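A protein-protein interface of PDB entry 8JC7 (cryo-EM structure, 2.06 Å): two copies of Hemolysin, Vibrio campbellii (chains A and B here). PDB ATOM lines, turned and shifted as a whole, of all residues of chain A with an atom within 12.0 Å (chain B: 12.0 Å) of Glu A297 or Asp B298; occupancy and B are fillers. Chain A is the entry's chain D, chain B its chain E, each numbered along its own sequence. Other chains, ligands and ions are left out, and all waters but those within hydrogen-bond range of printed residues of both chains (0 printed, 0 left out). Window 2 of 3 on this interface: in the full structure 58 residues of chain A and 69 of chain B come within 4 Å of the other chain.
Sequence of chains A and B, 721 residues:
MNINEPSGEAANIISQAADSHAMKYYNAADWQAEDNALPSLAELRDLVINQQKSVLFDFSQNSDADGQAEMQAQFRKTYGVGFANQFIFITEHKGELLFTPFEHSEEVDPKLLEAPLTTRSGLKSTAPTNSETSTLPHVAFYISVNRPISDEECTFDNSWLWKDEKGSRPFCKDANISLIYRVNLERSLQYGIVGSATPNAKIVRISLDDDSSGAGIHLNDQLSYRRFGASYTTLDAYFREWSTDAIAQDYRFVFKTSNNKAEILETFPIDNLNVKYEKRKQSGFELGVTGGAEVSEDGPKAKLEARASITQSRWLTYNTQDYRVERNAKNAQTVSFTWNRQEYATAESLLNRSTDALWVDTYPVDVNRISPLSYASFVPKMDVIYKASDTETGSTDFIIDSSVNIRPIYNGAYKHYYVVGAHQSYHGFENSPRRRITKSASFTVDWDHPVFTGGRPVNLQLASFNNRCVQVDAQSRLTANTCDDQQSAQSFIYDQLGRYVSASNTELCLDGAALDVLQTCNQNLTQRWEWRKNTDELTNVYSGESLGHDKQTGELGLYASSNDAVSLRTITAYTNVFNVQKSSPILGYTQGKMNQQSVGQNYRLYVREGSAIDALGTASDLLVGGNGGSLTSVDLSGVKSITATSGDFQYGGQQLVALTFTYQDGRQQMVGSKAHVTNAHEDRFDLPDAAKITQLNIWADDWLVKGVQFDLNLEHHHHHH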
ATOM      1  N   ALA A 293     -27.684   9.970 -15.819  1.00  0.00           N
ATOM      2  CA  ALA A 293     -28.885   9.159 -15.983  1.00  0.00           C
ATOM      3  C   ALA A 293     -28.516   7.713 -15.694  1.00  0.00           C
ATOM      4  O   ALA A 293     -27.896   7.051 -16.530  1.00  0.00           O
ATOM      5  CB  ALA A 293     -29.466   9.303 -17.387  1.00  0.00           C
ATOM      6  N   GLU A 294     -28.892   7.226 -14.520  1.00  0.00           N
ATOM      7  CA  GLU A 294     -28.590   5.865 -14.106  1.00  0.00           C
ATOM      8  C   GLU A 294     -29.852   5.024 -14.224  1.00  0.00           C
ATOM      9  O   GLU A 294     -30.896   5.384 -13.670  1.00  0.00           O
ATOM     10  CB  GLU A 294     -28.056   5.839 -12.676  1.00  0.00           C
ATOM     11  CG  GLU A 294     -27.828   4.450 -12.124  1.00  0.00           C
ATOM     12  CD  GLU A 294     -27.201   4.477 -10.746  1.00  0.00           C
ATOM     13  OE1 GLU A 294     -26.502   5.462 -10.431  1.00  0.00           O
ATOM     14  OE2 GLU A 294     -27.409   3.517  -9.976  1.00  0.00           O
ATOM     15  N   VAL A 295     -29.760   3.912 -14.944  1.00  0.00           N
ATOM     16  CA  VAL A 295     -30.878   2.998 -15.132  1.00  0.00           C
ATOM     17  C   VAL A 295     -30.491   1.647 -14.549  1.00  0.00           C
ATOM     18  O   VAL A 295     -29.331   1.231 -14.644  1.00  0.00           O
ATOM     19  CB  VAL A 295     -31.281   2.882 -16.614  1.00  0.00           C
ATOM     20  CG1 VAL A 295     -30.424   1.871 -17.348  1.00  0.00           C
ATOM     21  CG2 VAL A 295     -32.745   2.513 -16.731  1.00  0.00           C
ATOM     22  N   SER A 296     -31.448   0.992 -13.904  1.00  0.00           N
ATOM     23  CA  SER A 296     -31.217  -0.305 -13.287  1.00  0.00           C
ATOM     24  C   SER A 296     -32.569  -0.953 -13.017  1.00  0.00           C
ATOM     25  O   SER A 296     -33.608  -0.474 -13.477  1.00  0.00           O
ATOM     26  CB  SER A 296     -30.386  -0.162 -12.007  1.00  0.00           C
ATOM     27  OG  SER A 296     -31.216   0.063 -10.884  1.00  0.00           O
ATOM     28  N   GLU A 297     -32.548  -2.053 -12.264  1.00  0.00           N
ATOM     29  CA  GLU A 297     -33.793  -2.707 -11.883  1.00  0.00           C
ATOM     30  C   GLU A 297     -34.627  -1.831 -10.957  1.00  0.00           C
ATOM     31  O   GLU A 297     -35.856  -1.953 -10.934  1.00  0.00           O
ATOM     32  CB  GLU A 297     -33.491  -4.053 -11.221  1.00  0.00           C
ATOM     33  CG  GLU A 297     -32.989  -3.946  -9.789  1.00  0.00           C
ATOM     34  CD  GLU A 297     -31.481  -3.792  -9.704  1.00  0.00           C
ATOM     35  OE1 GLU A 297     -30.851  -4.536  -8.924  1.00  0.00           O
ATOM     36  OE2 GLU A 297     -30.923  -2.936 -10.420  1.00  0.00           O
ATOM     37  N   ASP A 298     -33.982  -0.946 -10.193  1.00  0.00           N
ATOM     38  CA  ASP A 298     -34.721  -0.086  -9.276  1.00  0.00           C
ATOM     39  C   ASP A 298     -35.585   0.915 -10.032  1.00  0.00           C
ATOM     40  O   ASP A 298     -36.720   1.191  -9.630  1.00  0.00           O
ATOM     41  CB  ASP A 298     -33.749   0.637  -8.345  1.00  0.00           C
ATOM     42  CG  ASP A 298     -32.954  -0.318  -7.484  1.00  0.00           C
ATOM     43  OD1 ASP A 298     -33.291  -1.520  -7.465  1.00  0.00           O
ATOM     44  OD2 ASP A 298     -31.993   0.128  -6.825  1.00  0.00           O
ATOM     45  N   GLY A 299     -35.070   1.464 -11.126  1.00  0.00           N
ATOM     46  CA  GLY A 299     -35.796   2.435 -11.906  1.00  0.00           C
ATOM     47  C   GLY A 299     -34.908   3.573 -12.353  1.00  0.00           C
ATOM     48  O   GLY A 299     -33.800   3.761 -11.843  1.00  0.00           O
ATOM     49  N   PRO A 300     -35.376   4.348 -13.328  1.00  0.00           N
ATOM     50  CA  PRO A 300     -34.573   5.473 -13.822  1.00  0.00           C
ATOM     51  C   PRO A 300     -34.223   6.441 -12.704  1.00  0.00           C
ATOM     52  O   PRO A 300     -35.046   6.752 -11.841  1.00  0.00           O
ATOM     53  CB  PRO A 300     -35.479   6.131 -14.867  1.00  0.00           C
ATOM     54  CG  PRO A 300     -36.473   5.105 -15.248  1.00  0.00           C
ATOM     55  CD  PRO A 300     -36.541   4.060 -14.179  1.00  0.00           C
ATOM     56  N   LYS A 301     -32.981   6.915 -12.730  1.00  0.00           N
ATOM     57  CA  LYS A 301     -32.471   7.842 -11.734  1.00  0.00           C
ATOM     58  C   LYS A 301     -31.716   8.947 -12.452  1.00  0.00           C
ATOM     59  O   LYS A 301     -30.829   8.664 -13.262  1.00  0.00           O
ATOM     60  CB  LYS A 301     -31.557   7.126 -10.738  1.00  0.00           C
ATOM     61  CG  LYS A 301     -30.988   8.016  -9.662  1.00  0.00           C
ATOM     62  CD  LYS A 301     -29.651   7.482  -9.182  1.00  0.00           C
ATOM     63  CE  LYS A 301     -29.764   6.036  -8.738  1.00  0.00           C
ATOM     64  NZ  LYS A 301     -30.497   5.907  -7.449  1.00  0.00           N
ATOM     65  N   GLY B 292     -20.933   4.064 -17.849  1.00  0.00           N
ATOM     66  CA  GLY B 292     -20.573   3.073 -16.855  1.00  0.00           C
ATOM     67  C   GLY B 292     -21.502   1.877 -16.902  1.00  0.00           C
ATOM     68  O   GLY B 292     -22.679   1.999 -17.235  1.00  0.00           O
ATOM     69  N   ALA B 293     -20.955   0.713 -16.566  1.00  0.00           N
ATOM     70  CA  ALA B 293     -21.710  -0.534 -16.516  1.00  0.00           C
ATOM     71  C   ALA B 293     -21.290  -1.286 -15.265  1.00  0.00           C
ATOM     72  O   ALA B 293     -20.188  -1.837 -15.210  1.00  0.00           O
ATOM     73  CB  ALA B 293     -21.468  -1.377 -17.765  1.00  0.00           C
ATOM     74  N   GLU B 294     -22.163  -1.312 -14.266  1.00  0.00           N
ATOM     75  CA  GLU B 294     -21.891  -1.994 -13.009  1.00  0.00           C
ATOM     76  C   GLU B 294     -22.688  -3.289 -12.970  1.00  0.00           C
ATOM     77  O   GLU B 294     -23.913  -3.272 -13.124  1.00  0.00           O
ATOM     78  CB  GLU B 294     -22.247  -1.101 -11.823  1.00  0.00           C
ATOM     79  CG  GLU B 294     -22.105  -1.771 -10.475  1.00  0.00           C
ATOM     80  CD  GLU B 294     -22.361  -0.814  -9.330  1.00  0.00           C
ATOM     81  OE1 GLU B 294     -22.145   0.403  -9.514  1.00  0.00           O
ATOM     82  OE2 GLU B 294     -22.783  -1.272  -8.249  1.00  0.00           O
ATOM     83  N   VAL B 295     -21.996  -4.404 -12.770  1.00  0.00           N
ATOM     84  CA  VAL B 295     -22.617  -5.722 -12.714  1.00  0.00           C
ATOM     85  C   VAL B 295     -22.349  -6.322 -11.344  1.00  0.00           C
ATOM     86  O   VAL B 295     -21.196  -6.399 -10.907  1.00  0.00           O
ATOM     87  CB  VAL B 295     -22.099  -6.642 -13.836  1.00  0.00           C
ATOM     88  CG1 VAL B 295     -20.587  -6.569 -13.939  1.00  0.00           C
ATOM     89  CG2 VAL B 295     -22.541  -8.070 -13.591  1.00  0.00           C
ATOM     90  N   SER B 296     -23.412  -6.738 -10.666  1.00  0.00           N
ATOM     91  CA  SER B 296     -23.296  -7.327  -9.343  1.00  0.00           C
ATOM     92  C   SER B 296     -24.441  -8.317  -9.158  1.00  0.00           C
ATOM     93  O   SER B 296     -25.147  -8.660 -10.110  1.00  0.00           O
ATOM     94  CB  SER B 296     -23.297  -6.242  -8.262  1.00  0.00           C
ATOM     95  OG  SER B 296     -24.615  -5.936  -7.850  1.00  0.00           O
ATOM     96  N   GLU B 297     -24.621  -8.777  -7.920  1.00  0.00           N
ATOM     97  CA  GLU B 297     -25.711  -9.698  -7.626  1.00  0.00           C
ATOM     98  C   GLU B 297     -27.070  -9.034  -7.798  1.00  0.00           C
ATOM     99  O   GLU B 297     -28.059  -9.716  -8.088  1.00  0.00           O
ATOM    100  CB  GLU B 297     -25.559 -10.252  -6.208  1.00  0.00           C
ATOM    101  CG  GLU B 297     -25.967  -9.280  -5.110  1.00  0.00           C
ATOM    102  CD  GLU B 297     -24.825  -8.387  -4.663  1.00  0.00           C
ATOM    103  OE1 GLU B 297     -24.595  -8.279  -3.441  1.00  0.00           O
ATOM    104  OE2 GLU B 297     -24.151  -7.794  -5.531  1.00  0.00           O
ATOM    105  N   ASP B 298     -27.141  -7.713  -7.629  1.00  0.00           N
ATOM    106  CA  ASP B 298     -28.413  -7.016  -7.775  1.00  0.00           C
ATOM    107  C   ASP B 298     -28.899  -7.051  -9.218  1.00  0.00           C
ATOM    108  O   ASP B 298     -30.098  -7.222  -9.472  1.00  0.00           O
ATOM    109  CB  ASP B 298     -28.281  -5.577  -7.285  1.00  0.00           C
ATOM    110  CG  ASP B 298     -27.925  -5.496  -5.816  1.00  0.00           C
ATOM    111  OD1 ASP B 298     -27.977  -6.540  -5.135  1.00  0.00           O
ATOM    112  OD2 ASP B 298     -27.593  -4.391  -5.342  1.00  0.00           O
ATOM    113  N   GLY B 299     -27.990  -6.896 -10.173  1.00  0.00           N
ATOM    114  CA  GLY B 299     -28.346  -6.900 -11.569  1.00  0.00           C
ATOM    115  C   GLY B 299     -27.597  -5.839 -12.344  1.00  0.00           C
ATOM    116  O   GLY B 299     -27.028  -4.906 -11.770  1.00  0.00           O
ATOM    117  N   PRO B 300     -27.563  -5.979 -13.667  1.00  0.00           N
ATOM    118  CA  PRO B 300     -26.874  -4.987 -14.496  1.00  0.00           C
ATOM    119  C   PRO B 300     -27.371  -3.579 -14.218  1.00  0.00           C
ATOM    120  O   PRO B 300     -28.571  -3.332 -14.091  1.00  0.00           O
ATOM    121  CB  PRO B 300     -27.223  -5.426 -15.922  1.00  0.00           C
ATOM    122  CG  PRO B 300     -27.561  -6.898 -15.815  1.00  0.00           C
ATOM    123  CD  PRO B 300     -27.643  -7.276 -14.354  1.00  0.00           C
ATOM    124  N   LYS B 301     -26.425  -2.650 -14.123  1.00  0.00           N
ATOM    125  CA  LYS B 301     -26.718  -1.249 -13.862  1.00  0.00           C
ATOM    126  C   LYS B 301     -25.907  -0.404 -14.827  1.00  0.00           C
ATOM    127  O   LYS B 301     -24.686  -0.553 -14.903  1.00  0.00           O
ATOM    128  CB  LYS B 301     -26.387  -0.881 -12.415  1.00  0.00           C
ATOM    129  CG  LYS B 301     -26.676   0.556 -12.057  1.00  0.00           C
ATOM    130  CD  LYS B 301     -25.749   1.029 -10.954  1.00  0.00           C
ATOM    131  CE  LYS B 301     -25.816   0.111  -9.748  1.00  0.00           C
ATOM    132  NZ  LYS B 301     -27.095   0.266  -9.006  1.00  0.00           N
ATOM    133  N   ALA B 302     -26.579   0.476 -15.560  1.00  0.00           N
ATOM    134  CA  ALA B 302     -25.944   1.285 -16.586  1.00  0.00           C
ATOM    135  C   ALA B 302     -25.990   2.751 -16.190  1.00  0.00           C
ATOM    136  O   ALA B 302     -26.980   3.222 -15.627  1.00  0.00           O
ATOM    137  CB  ALA B 302     -26.616   1.088 -17.942  1.00  0.00           C
ATOM    138  N   LYS B 303     -24.908   3.466 -16.485  1.00  0.00           N
ATOM    139  CA  LYS B 303     -24.774   4.879 -16.168  1.00  0.00           C
ATOM    140  C   LYS B 303     -24.394   5.646 -17.422  1.00  0.00           C
ATOM    141  O   LYS B 303     -23.634   5.150 -18.257  1.00  0.00           O
ATOM    142  CB  LYS B 303     -23.720   5.113 -15.095  1.00  0.00           C
ATOM    143  CG  LYS B 303     -24.269   5.659 -13.802  1.00  0.00           C
ATOM    144  CD  LYS B 303     -23.223   5.604 -12.713  1.00  0.00           C
ATOM    145  CE  LYS B 303     -23.362   4.347 -11.879  1.00  0.00           C
ATOM    146  NZ  LYS B 303     -22.355   4.312 -10.786  1.00  0.00           N
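The backbone NH (N) of Glu A294 lies within hydrogen-bond range of the backbone carbonyl oxygen (O) of Lys A301.
The backbone NH (N) of Glu B294 sits at hydrogen-bond distance from the backbone carbonyl oxygen (O) of Lys B301, at 2.7 Å.
N of Lys B303 is in hydrogen-bond range of O of Gly B292, 2.8 Å away.
The backbone NH (N) of Asp B298 is in hydrogen-bond range of the side-chain hydroxyl (OG) of Ser B296.
OG of Ser A296 sits at hydrogen-bond distance from N of Asp A298.
OG of Ser A296 lies within hydrogen-bond range of OE2 of Glu A297 (3.0 Å).
The side-chain carboxylate (OE2) of Glu A294 is in salt-bridge range of the side-chain amino group (NZ) of Lys B301, at 3.4 Å.
The backbone carbonyl oxygen (O) of Ala B302 sits at hydrogen-bond distance from the backbone NH (N) of Val A295 (2.9 Å).
The side-chain carboxylate of Glu A297 sits close to the backbone carbonyl oxygen of Asp B298 (2.8 Å).
Val A295 touches Lys B301, but with the chains exchanged Lys A301 does not touch Val B295 (13.6 Å).
Ser A296 touches Lys B301, but with the chains exchanged Lys A301 does not touch Ser B296 (13.1 Å).
Glu A297 touches Asp B298, but with the chains exchanged Asp A298 does not touch Glu B297 (9.7 Å).
Glu A297 touches Gly B299, but with the chains exchanged Gly A299 does not touch Glu B297 (13.5 Å).
Printed residues of chain B that touch a printed residue of chain A: Asp B298, Gly B299, Lys B301, Ala B302 and Lys B303.
Hydrophobic or aromatic side chains of chain B within 4 Å of the printed part of chain A: Ala B302.
Among the printed residues, Asp or Glu carboxylates within 4 Å of a Lys or Arg side-chain nitrogen of the other chain: Glu A294 with Lys B301 (3.4 Å).
Of the printed residues of chain B, Ala A293 touches Lys B303.
Printed residues of chain B within 4 Å of Glu A294: Lys B301 (3.1 Å), Ala B302 (3.4 Å) and Lys B303 (3.6 Å).
Of the printed residues of chain B, Val A295 touches Lys B301 (3.7 Å) and Ala B302 (2.9 Å).
Ser A296 touches just one residue of chain B: Lys B301 (3.8 Å).
Of chain B, only Asp B298 (2.8 Å) and Gly B299 (3.9 Å) come within 4 Å of Glu A297.
Asp A298 touches none of the printed residues of chain B.
No residue of chain B comes within 4 Å of Gly A299.
Gly B292 touches none of the printed residues of chain A.
Asp B298 touches one residue of chain A.
Gly B299 touches just one residue of chain A: Glu A297.
No residue of chain A comes within 4 Å of Pro B300.
Printed residues of chain A within 4 Å of Lys B301: Glu A294 (3.1 Å), Val A295 (3.7 Å) and Ser A296 (3.8 Å).
Of the printed residues of chain A, Ala B302 touches Glu A294 (3.4 Å) and Val A295 (2.9 Å).
Printed residues of chain A within 4 Å of Lys B303: Ala A293 and Glu A294.
The nearest residue of chain A that does not touch Asp B298 is Asp A298 (6.4 Å).
The nearest printed residue of chain B that does not touch Glu A294 is Glu B294 (6.1 Å).
Lys B303 touches Ala A293 (CA to O, 3.8 Å).
Glu A294 touches Ala B302.
Glu A294 touches Lys B303 (OE1 to CE, 3.6 Å).
Val A295 touches Lys B301.
Lys B301 touches Ser A296 (CG to CB, 3.8 Å).
Gly B299 touches Glu A297.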
